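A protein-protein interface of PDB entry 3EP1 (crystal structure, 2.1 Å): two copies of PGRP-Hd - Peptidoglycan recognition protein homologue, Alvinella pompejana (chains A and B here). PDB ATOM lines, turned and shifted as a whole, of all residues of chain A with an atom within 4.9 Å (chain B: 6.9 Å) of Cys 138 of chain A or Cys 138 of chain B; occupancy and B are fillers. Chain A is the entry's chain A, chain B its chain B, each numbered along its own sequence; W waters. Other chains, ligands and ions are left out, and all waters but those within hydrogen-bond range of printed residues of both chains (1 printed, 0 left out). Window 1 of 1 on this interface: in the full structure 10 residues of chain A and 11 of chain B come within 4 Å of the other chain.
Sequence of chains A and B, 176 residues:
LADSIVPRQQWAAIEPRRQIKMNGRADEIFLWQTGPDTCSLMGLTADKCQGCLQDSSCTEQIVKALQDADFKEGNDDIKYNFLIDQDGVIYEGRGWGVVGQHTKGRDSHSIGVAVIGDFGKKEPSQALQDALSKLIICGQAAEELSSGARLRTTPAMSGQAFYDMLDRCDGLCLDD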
ATOM      1  N   LYS A 134     -25.959 -18.158 -17.843  1.00  0.00           N
ATOM      2  CA  LYS A 134     -26.092 -18.244 -16.390  1.00  0.00           C
ATOM      3  C   LYS A 134     -26.676 -19.582 -15.941  1.00  0.00           C
ATOM      4  O   LYS A 134     -26.170 -20.199 -15.010  1.00  0.00           O
ATOM      5  CB  LYS A 134     -26.971 -17.102 -15.867  1.00  0.00           C
ATOM      6  CG  LYS A 134     -27.167 -17.094 -14.345  1.00  0.00           C
ATOM      7  CD  LYS A 134     -27.994 -15.882 -13.886  1.00  0.00           C
ATOM      8  CE  LYS A 134     -29.383 -15.911 -14.512  1.00  0.00           C
ATOM      9  NZ  LYS A 134     -30.086 -14.608 -14.432  1.00  0.00           N
ATOM     10  N   LEU A 135     -27.746 -20.021 -16.601  1.00  0.00           N
ATOM     11  CA  LEU A 135     -28.389 -21.281 -16.246  1.00  0.00           C
ATOM     12  C   LEU A 135     -27.395 -22.448 -16.232  1.00  0.00           C
ATOM     13  O   LEU A 135     -27.358 -23.253 -15.308  1.00  0.00           O
ATOM     14  CB  LEU A 135     -29.525 -21.574 -17.230  1.00  0.00           C
ATOM     15  CG  LEU A 135     -30.232 -22.924 -17.086  1.00  0.00           C
ATOM     16  CD1 LEU A 135     -30.917 -23.001 -15.739  1.00  0.00           C
ATOM     17  CD2 LEU A 135     -31.242 -23.106 -18.196  1.00  0.00           C
ATOM     18  N   ILE A 136     -26.588 -22.533 -17.273  1.00  0.00           N
ATOM     19  CA  ILE A 136     -25.614 -23.603 -17.386  1.00  0.00           C
ATOM     20  C   ILE A 136     -24.538 -23.511 -16.304  1.00  0.00           C
ATOM     21  O   ILE A 136     -24.259 -24.474 -15.591  1.00  0.00           O
ATOM     22  CB  ILE A 136     -24.955 -23.557 -18.766  1.00  0.00           C
ATOM     23  CG1 ILE A 136     -26.041 -23.689 -19.849  1.00  0.00           C
ATOM     24  CG2 ILE A 136     -23.874 -24.641 -18.860  1.00  0.00           C
ATOM     25  CD1 ILE A 136     -25.574 -23.406 -21.269  1.00  0.00           C
ATOM     26  N   ILE A 137     -23.944 -22.335 -16.177  1.00  0.00           N
ATOM     27  CA  ILE A 137     -22.904 -22.141 -15.193  1.00  0.00           C
ATOM     28  C   ILE A 137     -23.430 -22.435 -13.785  1.00  0.00           C
ATOM     29  O   ILE A 137     -22.745 -23.072 -12.978  1.00  0.00           O
ATOM     30  CB  ILE A 137     -22.315 -20.719 -15.324  1.00  0.00           C
ATOM     31  CG1 ILE A 137     -21.661 -20.585 -16.705  1.00  0.00           C
ATOM     32  CG2 ILE A 137     -21.276 -20.460 -14.234  1.00  0.00           C
ATOM     33  CD1 ILE A 137     -20.988 -19.254 -16.966  1.00  0.00           C
ATOM     34  N   CYS A 138     -24.655 -22.014 -13.491  1.00  0.00           N
ATOM     35  CA  CYS A 138     -25.206 -22.287 -12.172  1.00  0.00           C
ATOM     36  C   CYS A 138     -25.620 -23.755 -12.052  1.00  0.00           C
ATOM     37  O   CYS A 138     -25.661 -24.313 -10.956  1.00  0.00           O
ATOM     38  CB  CYS A 138     -26.378 -21.352 -11.877  1.00  0.00           C
ATOM     39  SG  CYS A 138     -25.855 -19.612 -11.655  1.00  0.00           S
ATOM     40  N   GLY A 139     -25.918 -24.385 -13.183  1.00  0.00           N
ATOM     41  CA  GLY A 139     -26.292 -25.786 -13.145  1.00  0.00           C
ATOM     42  C   GLY A 139     -25.048 -26.576 -12.782  1.00  0.00           C
ATOM     43  O   GLY A 139     -25.083 -27.498 -11.963  1.00  0.00           O
ATOM     44  N   GLN A 140     -23.937 -26.187 -13.399  1.00  0.00           N
ATOM     45  CA  GLN A 140     -22.645 -26.820 -13.172  1.00  0.00           C
ATOM     46  C   GLN A 140     -22.144 -26.612 -11.745  1.00  0.00           C
ATOM     47  O   GLN A 140     -21.659 -27.544 -11.112  1.00  0.00           O
ATOM     48  CB  GLN A 140     -21.631 -26.280 -14.187  1.00  0.00           C
ATOM     49  CG  GLN A 140     -21.768 -26.933 -15.566  1.00  0.00           C
ATOM     50  CD  GLN A 140     -21.181 -26.114 -16.700  1.00  0.00           C
ATOM     51  OE1 GLN A 140     -20.873 -26.648 -17.758  1.00  0.00           O
ATOM     52  NE2 GLN A 140     -21.042 -24.813 -16.492  1.00  0.00           N
ATOM     53  N   ALA A 141     -22.270 -25.390 -11.243  1.00  0.00           N
ATOM     54  CA  ALA A 141     -21.846 -25.079  -9.888  1.00  0.00           C
ATOM     55  C   ALA A 141     -22.616 -25.945  -8.894  1.00  0.00           C
ATOM     56  O   ALA A 141     -22.040 -26.446  -7.925  1.00  0.00           O
ATOM     57  CB  ALA A 141     -22.078 -23.602  -9.592  1.00  0.00           C
ATOM     58  N   ALA A 142     -23.914 -26.127  -9.147  1.00  0.00           N
ATOM     59  CA  ALA A 142     -24.774 -26.935  -8.278  1.00  0.00           C
ATOM     60  C   ALA A 142     -24.693 -28.429  -8.577  1.00  0.00           C
ATOM     61  O   ALA A 142     -25.448 -29.220  -8.017  1.00  0.00           O
ATOM     62  CB  ALA A 142     -26.215 -26.475  -8.388  1.00  0.00           C
ATOM     63  N   ILE B   5     -19.204 -26.503  -7.230  1.00  0.00           N
ATOM     64  CA  ILE B   5     -18.779 -26.155  -5.874  1.00  0.00           C
ATOM     65  C   ILE B   5     -18.281 -27.448  -5.225  1.00  0.00           C
ATOM     66  O   ILE B   5     -18.911 -28.496  -5.383  1.00  0.00           O
ATOM     67  CB  ILE B   5     -19.968 -25.599  -5.045  1.00  0.00           C
ATOM     68  CG1 ILE B   5     -20.417 -24.255  -5.623  1.00  0.00           C
ATOM     69  CG2 ILE B   5     -19.578 -25.463  -3.587  1.00  0.00           C
ATOM     70  CD1 ILE B   5     -21.618 -23.650  -4.936  1.00  0.00           C
ATOM     71  N   TRP B  96     -26.223 -23.978   1.590  1.00  0.00           N
ATOM     72  CA  TRP B  96     -27.401 -23.115   1.619  1.00  0.00           C
ATOM     73  C   TRP B  96     -28.429 -23.644   2.622  1.00  0.00           C
ATOM     74  O   TRP B  96     -28.437 -24.826   2.946  1.00  0.00           O
ATOM     75  CB  TRP B  96     -28.066 -23.061   0.240  1.00  0.00           C
ATOM     76  CG  TRP B  96     -27.211 -22.572  -0.886  1.00  0.00           C
ATOM     77  CD1 TRP B  96     -26.755 -23.309  -1.943  1.00  0.00           C
ATOM     78  CD2 TRP B  96     -26.787 -21.227  -1.123  1.00  0.00           C
ATOM     79  NE1 TRP B  96     -26.082 -22.503  -2.829  1.00  0.00           N
ATOM     80  CE2 TRP B  96     -26.085 -21.220  -2.350  1.00  0.00           C
ATOM     81  CE3 TRP B  96     -26.934 -20.024  -0.423  1.00  0.00           C
ATOM     82  CZ2 TRP B  96     -25.534 -20.057  -2.893  1.00  0.00           C
ATOM     83  CZ3 TRP B  96     -26.387 -18.867  -0.966  1.00  0.00           C
ATOM     84  CH2 TRP B  96     -25.695 -18.894  -2.189  1.00  0.00           C
ATOM     85  N   SER B 133     -18.668 -13.496  -6.993  1.00  0.00           N
ATOM     86  CA  SER B 133     -19.763 -12.955  -7.780  1.00  0.00           C
ATOM     87  C   SER B 133     -20.653 -14.097  -8.260  1.00  0.00           C
ATOM     88  O   SER B 133     -21.877 -13.997  -8.236  1.00  0.00           O
ATOM     89  CB  SER B 133     -19.205 -12.172  -8.970  1.00  0.00           C
ATOM     90  OG  SER B 133     -20.229 -11.804  -9.876  1.00  0.00           O
ATOM     91  N   LYS B 134     -20.022 -15.186  -8.690  1.00  0.00           N
ATOM     92  CA  LYS B 134     -20.736 -16.368  -9.167  1.00  0.00           C
ATOM     93  C   LYS B 134     -21.647 -16.967  -8.072  1.00  0.00           C
ATOM     94  O   LYS B 134     -22.846 -17.163  -8.280  1.00  0.00           O
ATOM     95  CB  LYS B 134     -19.713 -17.404  -9.647  1.00  0.00           C
ATOM     96  CG  LYS B 134     -20.266 -18.776  -9.962  1.00  0.00           C
ATOM     97  CD  LYS B 134     -19.128 -19.743 -10.305  1.00  0.00           C
ATOM     98  CE  LYS B 134     -19.583 -21.187 -10.223  1.00  0.00           C
ATOM     99  NZ  LYS B 134     -18.470 -22.155 -10.463  1.00  0.00           N
ATOM    100  N   LEU B 135     -21.062 -17.247  -6.913  1.00  0.00           N
ATOM    101  CA  LEU B 135     -21.786 -17.805  -5.774  1.00  0.00           C
ATOM    102  C   LEU B 135     -23.019 -16.974  -5.438  1.00  0.00           C
ATOM    103  O   LEU B 135     -24.064 -17.503  -5.054  1.00  0.00           O
ATOM    104  CB  LEU B 135     -20.858 -17.855  -4.561  1.00  0.00           C
ATOM    105  CG  LEU B 135     -21.408 -18.368  -3.235  1.00  0.00           C
ATOM    106  CD1 LEU B 135     -21.746 -19.844  -3.352  1.00  0.00           C
ATOM    107  CD2 LEU B 135     -20.363 -18.154  -2.142  1.00  0.00           C
ATOM    108  N   ILE B 136     -22.891 -15.665  -5.587  1.00  0.00           N
ATOM    109  CA  ILE B 136     -23.989 -14.758  -5.299  1.00  0.00           C
ATOM    110  C   ILE B 136     -25.075 -14.852  -6.369  1.00  0.00           C
ATOM    111  O   ILE B 136     -26.256 -15.043  -6.063  1.00  0.00           O
ATOM    112  CB  ILE B 136     -23.484 -13.299  -5.213  1.00  0.00           C
ATOM    113  CG1 ILE B 136     -22.547 -13.155  -4.007  1.00  0.00           C
ATOM    114  CG2 ILE B 136     -24.673 -12.333  -5.126  1.00  0.00           C
ATOM    115  CD1 ILE B 136     -22.095 -11.742  -3.738  1.00  0.00           C
ATOM    116  N   ILE B 137     -24.667 -14.717  -7.624  1.00  0.00           N
ATOM    117  CA  ILE B 137     -25.598 -14.781  -8.739  1.00  0.00           C
ATOM    118  C   ILE B 137     -26.339 -16.111  -8.765  1.00  0.00           C
ATOM    119  O   ILE B 137     -27.560 -16.146  -8.900  1.00  0.00           O
ATOM    120  CB  ILE B 137     -24.869 -14.579 -10.074  1.00  0.00           C
ATOM    121  CG1 ILE B 137     -24.136 -13.234 -10.053  1.00  0.00           C
ATOM    122  CG2 ILE B 137     -25.864 -14.605 -11.223  1.00  0.00           C
ATOM    123  CD1 ILE B 137     -23.330 -12.939 -11.301  1.00  0.00           C
ATOM    124  N   CYS B 138     -25.608 -17.205  -8.620  1.00  0.00           N
ATOM    125  CA  CYS B 138     -26.243 -18.511  -8.635  1.00  0.00           C
ATOM    126  C   CYS B 138     -27.191 -18.711  -7.448  1.00  0.00           C
ATOM    127  O   CYS B 138     -28.275 -19.266  -7.604  1.00  0.00           O
ATOM    128  CB  CYS B 138     -25.183 -19.616  -8.681  1.00  0.00           C
ATOM    129  SG  CYS B 138     -24.333 -19.726 -10.296  1.00  0.00           S
ATOM    130  N   GLY B 139     -26.785 -18.247  -6.270  1.00  0.00           N
ATOM    131  CA  GLY B 139     -27.626 -18.390  -5.097  1.00  0.00           C
ATOM    132  C   GLY B 139     -28.938 -17.650  -5.276  1.00  0.00           C
ATOM    133  O   GLY B 139     -30.002 -18.115  -4.859  1.00  0.00           O
ATOM    134  N   GLN B 140     -28.855 -16.481  -5.895  1.00  0.00           N
ATOM    135  CA  GLN B 140     -30.037 -15.678  -6.146  1.00  0.00           C
ATOM    136  C   GLN B 140     -30.930 -16.357  -7.194  1.00  0.00           C
ATOM    137  O   GLN B 140     -32.153 -16.411  -7.043  1.00  0.00           O
ATOM    138  CB  GLN B 140     -29.616 -14.276  -6.597  1.00  0.00           C
ATOM    139  CG  GLN B 140     -29.039 -13.435  -5.446  1.00  0.00           C
ATOM    140  CD  GLN B 140     -28.497 -12.089  -5.894  1.00  0.00           C
ATOM    141  OE1 GLN B 140     -28.531 -11.114  -5.138  1.00  0.00           O
ATOM    142  NE2 GLN B 140     -27.982 -12.028  -7.114  1.00  0.00           N
ATOM    143  N   ALA B 141     -30.308 -16.901  -8.239  1.00  0.00           N
ATOM    144  CA  ALA B 141     -31.053 -17.579  -9.290  1.00  0.00           C
ATOM    145  C   ALA B 141     -31.888 -18.700  -8.693  1.00  0.00           C
ATOM    146  O   ALA B 141     -33.015 -18.946  -9.128  1.00  0.00           O
ATOM    147  CB  ALA B 141     -30.095 -18.143 -10.342  1.00  0.00           C
ATOM    148  N   ALA B 142     -31.340 -19.376  -7.690  1.00  0.00           N
ATOM    149  CA  ALA B 142     -32.048 -20.486  -7.070  1.00  0.00           C
ATOM    150  C   ALA B 142     -32.849 -20.105  -5.822  1.00  0.00           C
ATOM    151  O   ALA B 142     -33.212 -20.968  -5.018  1.00  0.00           O
ATOM    152  CB  ALA B 142     -31.070 -21.599  -6.747  1.00  0.00           C
ATOM    153  N   GLU B 143     -33.129 -18.816  -5.673  1.00  0.00           N
ATOM    154  CA  GLU B 143     -33.905 -18.323  -4.539  1.00  0.00           C
ATOM    155  C   GLU B 143     -33.308 -18.624  -3.168  1.00  0.00           C
ATOM    156  O   GLU B 143     -34.038 -18.692  -2.179  1.00  0.00           O
ATOM    157  CB  GLU B 143     -35.330 -18.883  -4.589  1.00  0.00           C
ATOM    158  CG  GLU B 143     -36.008 -18.725  -5.938  1.00  0.00           C
ATOM    159  CD  GLU B 143     -37.519 -18.844  -5.847  1.00  0.00           C
ATOM    160  OE1 GLU B 143     -38.154 -17.890  -5.348  1.00  0.00           O
ATOM    161  OE2 GLU B 143     -38.077 -19.890  -6.267  1.00  0.00           O
ATOM    162  N   GLU B 144     -31.992 -18.804  -3.104  1.00  0.00           N
ATOM    163  CA  GLU B 144     -31.326 -19.068  -1.831  1.00  0.00           C
ATOM    164  C   GLU B 144     -30.996 -17.730  -1.188  1.00  0.00           C
ATOM    165  O   GLU B 144     -30.998 -17.598   0.035  1.00  0.00           O
ATOM    166  CB  GLU B 144     -30.043 -19.881  -2.050  1.00  0.00           C
ATOM    167  CG  GLU B 144     -30.280 -21.339  -2.448  1.00  0.00           C
ATOM    168  CD  GLU B 144     -30.947 -22.146  -1.347  1.00  0.00           C
ATOM    169  OE1 GLU B 144     -31.184 -23.351  -1.546  1.00  0.00           O
ATOM    170  OE2 GLU B 144     -31.233 -21.577  -0.276  1.00  0.00           O
ATOM    171  N   LEU B 145     -30.717 -16.744  -2.041  1.00  0.00           N
ATOM    172  CA  LEU B 145     -30.400 -15.373  -1.625  1.00  0.00           C
ATOM    173  C   LEU B 145     -31.399 -14.400  -2.246  1.00  0.00           C
ATOM    174  O   LEU B 145     -31.803 -14.573  -3.398  1.00  0.00           O
ATOM    175  CB  LEU B 145     -28.999 -14.965  -2.096  1.00  0.00           C
ATOM    176  CG  LEU B 145     -27.756 -15.378  -1.311  1.00  0.00           C
ATOM    177  CD1 LEU B 145     -26.520 -14.991  -2.119  1.00  0.00           C
ATOM    178  CD2 LEU B 145     -27.752 -14.693   0.060  1.00  0.00           C
HETATM  179  O   HOH W   1     -19.994 -22.951 -12.617  1.00  0.00           O
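Lys 134 of chain A touches Ile 137 of chain B, but with the chains exchanged Ile 137 of chain A does not touch Lys 134 of chain B (4.4 Å).
Cys 138 of chain B touches its own counterpart, Cys 138 of chain A.
Ala 141 of chain A touches Lys 134 of chain B, but with the chains exchanged Lys 134 of chain A does not touch Ala 141 of chain B (4.7 Å).
The side-chain sulfur (SG) of Cys 138 of chain A is disulfide-bonded to the side-chain sulfur (SG) of Cys 138 of chain B, at 2.0 Å.
The backbone NH (N) of Ile 5 of chain B is in hydrogen-bond range of the backbone carbonyl oxygen (O) of Ala 141 of chain A, 2.9 Å away.
Of chain B, only Cys 138 comes within 4 Å of Cys 138 of chain A.
Of the printed residues of chain A, Ile 137 of chain B touches Lys 134.
Of the printed residues of chain B, Ala 141 of chain A touches Ile 5 and Lys 134.
The nearest printed residue of chain A that does not touch Ile 5 of chain B is Gln 140 of chain A (4.7 Å).
Hydrophobic or aromatic side chains of chain A that line the printed part of chain B: Ala 141.
Printed residues of chain B that touch a printed residue of chain A: Ile 5, Lys 134, Ile 137 and Cys 138.
Among the printed residues, merely in contact across the chains: Ala 141 of chain A with Lys 134 of chain B (3.5 Å) and Lys 134 of chain A with Ile 137 of chain B (3.6 Å).
Water W1 bridges NZ of Lys 134 of chain B (2.8 Å) and O of Ile 137 of chain A (2.8 Å).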
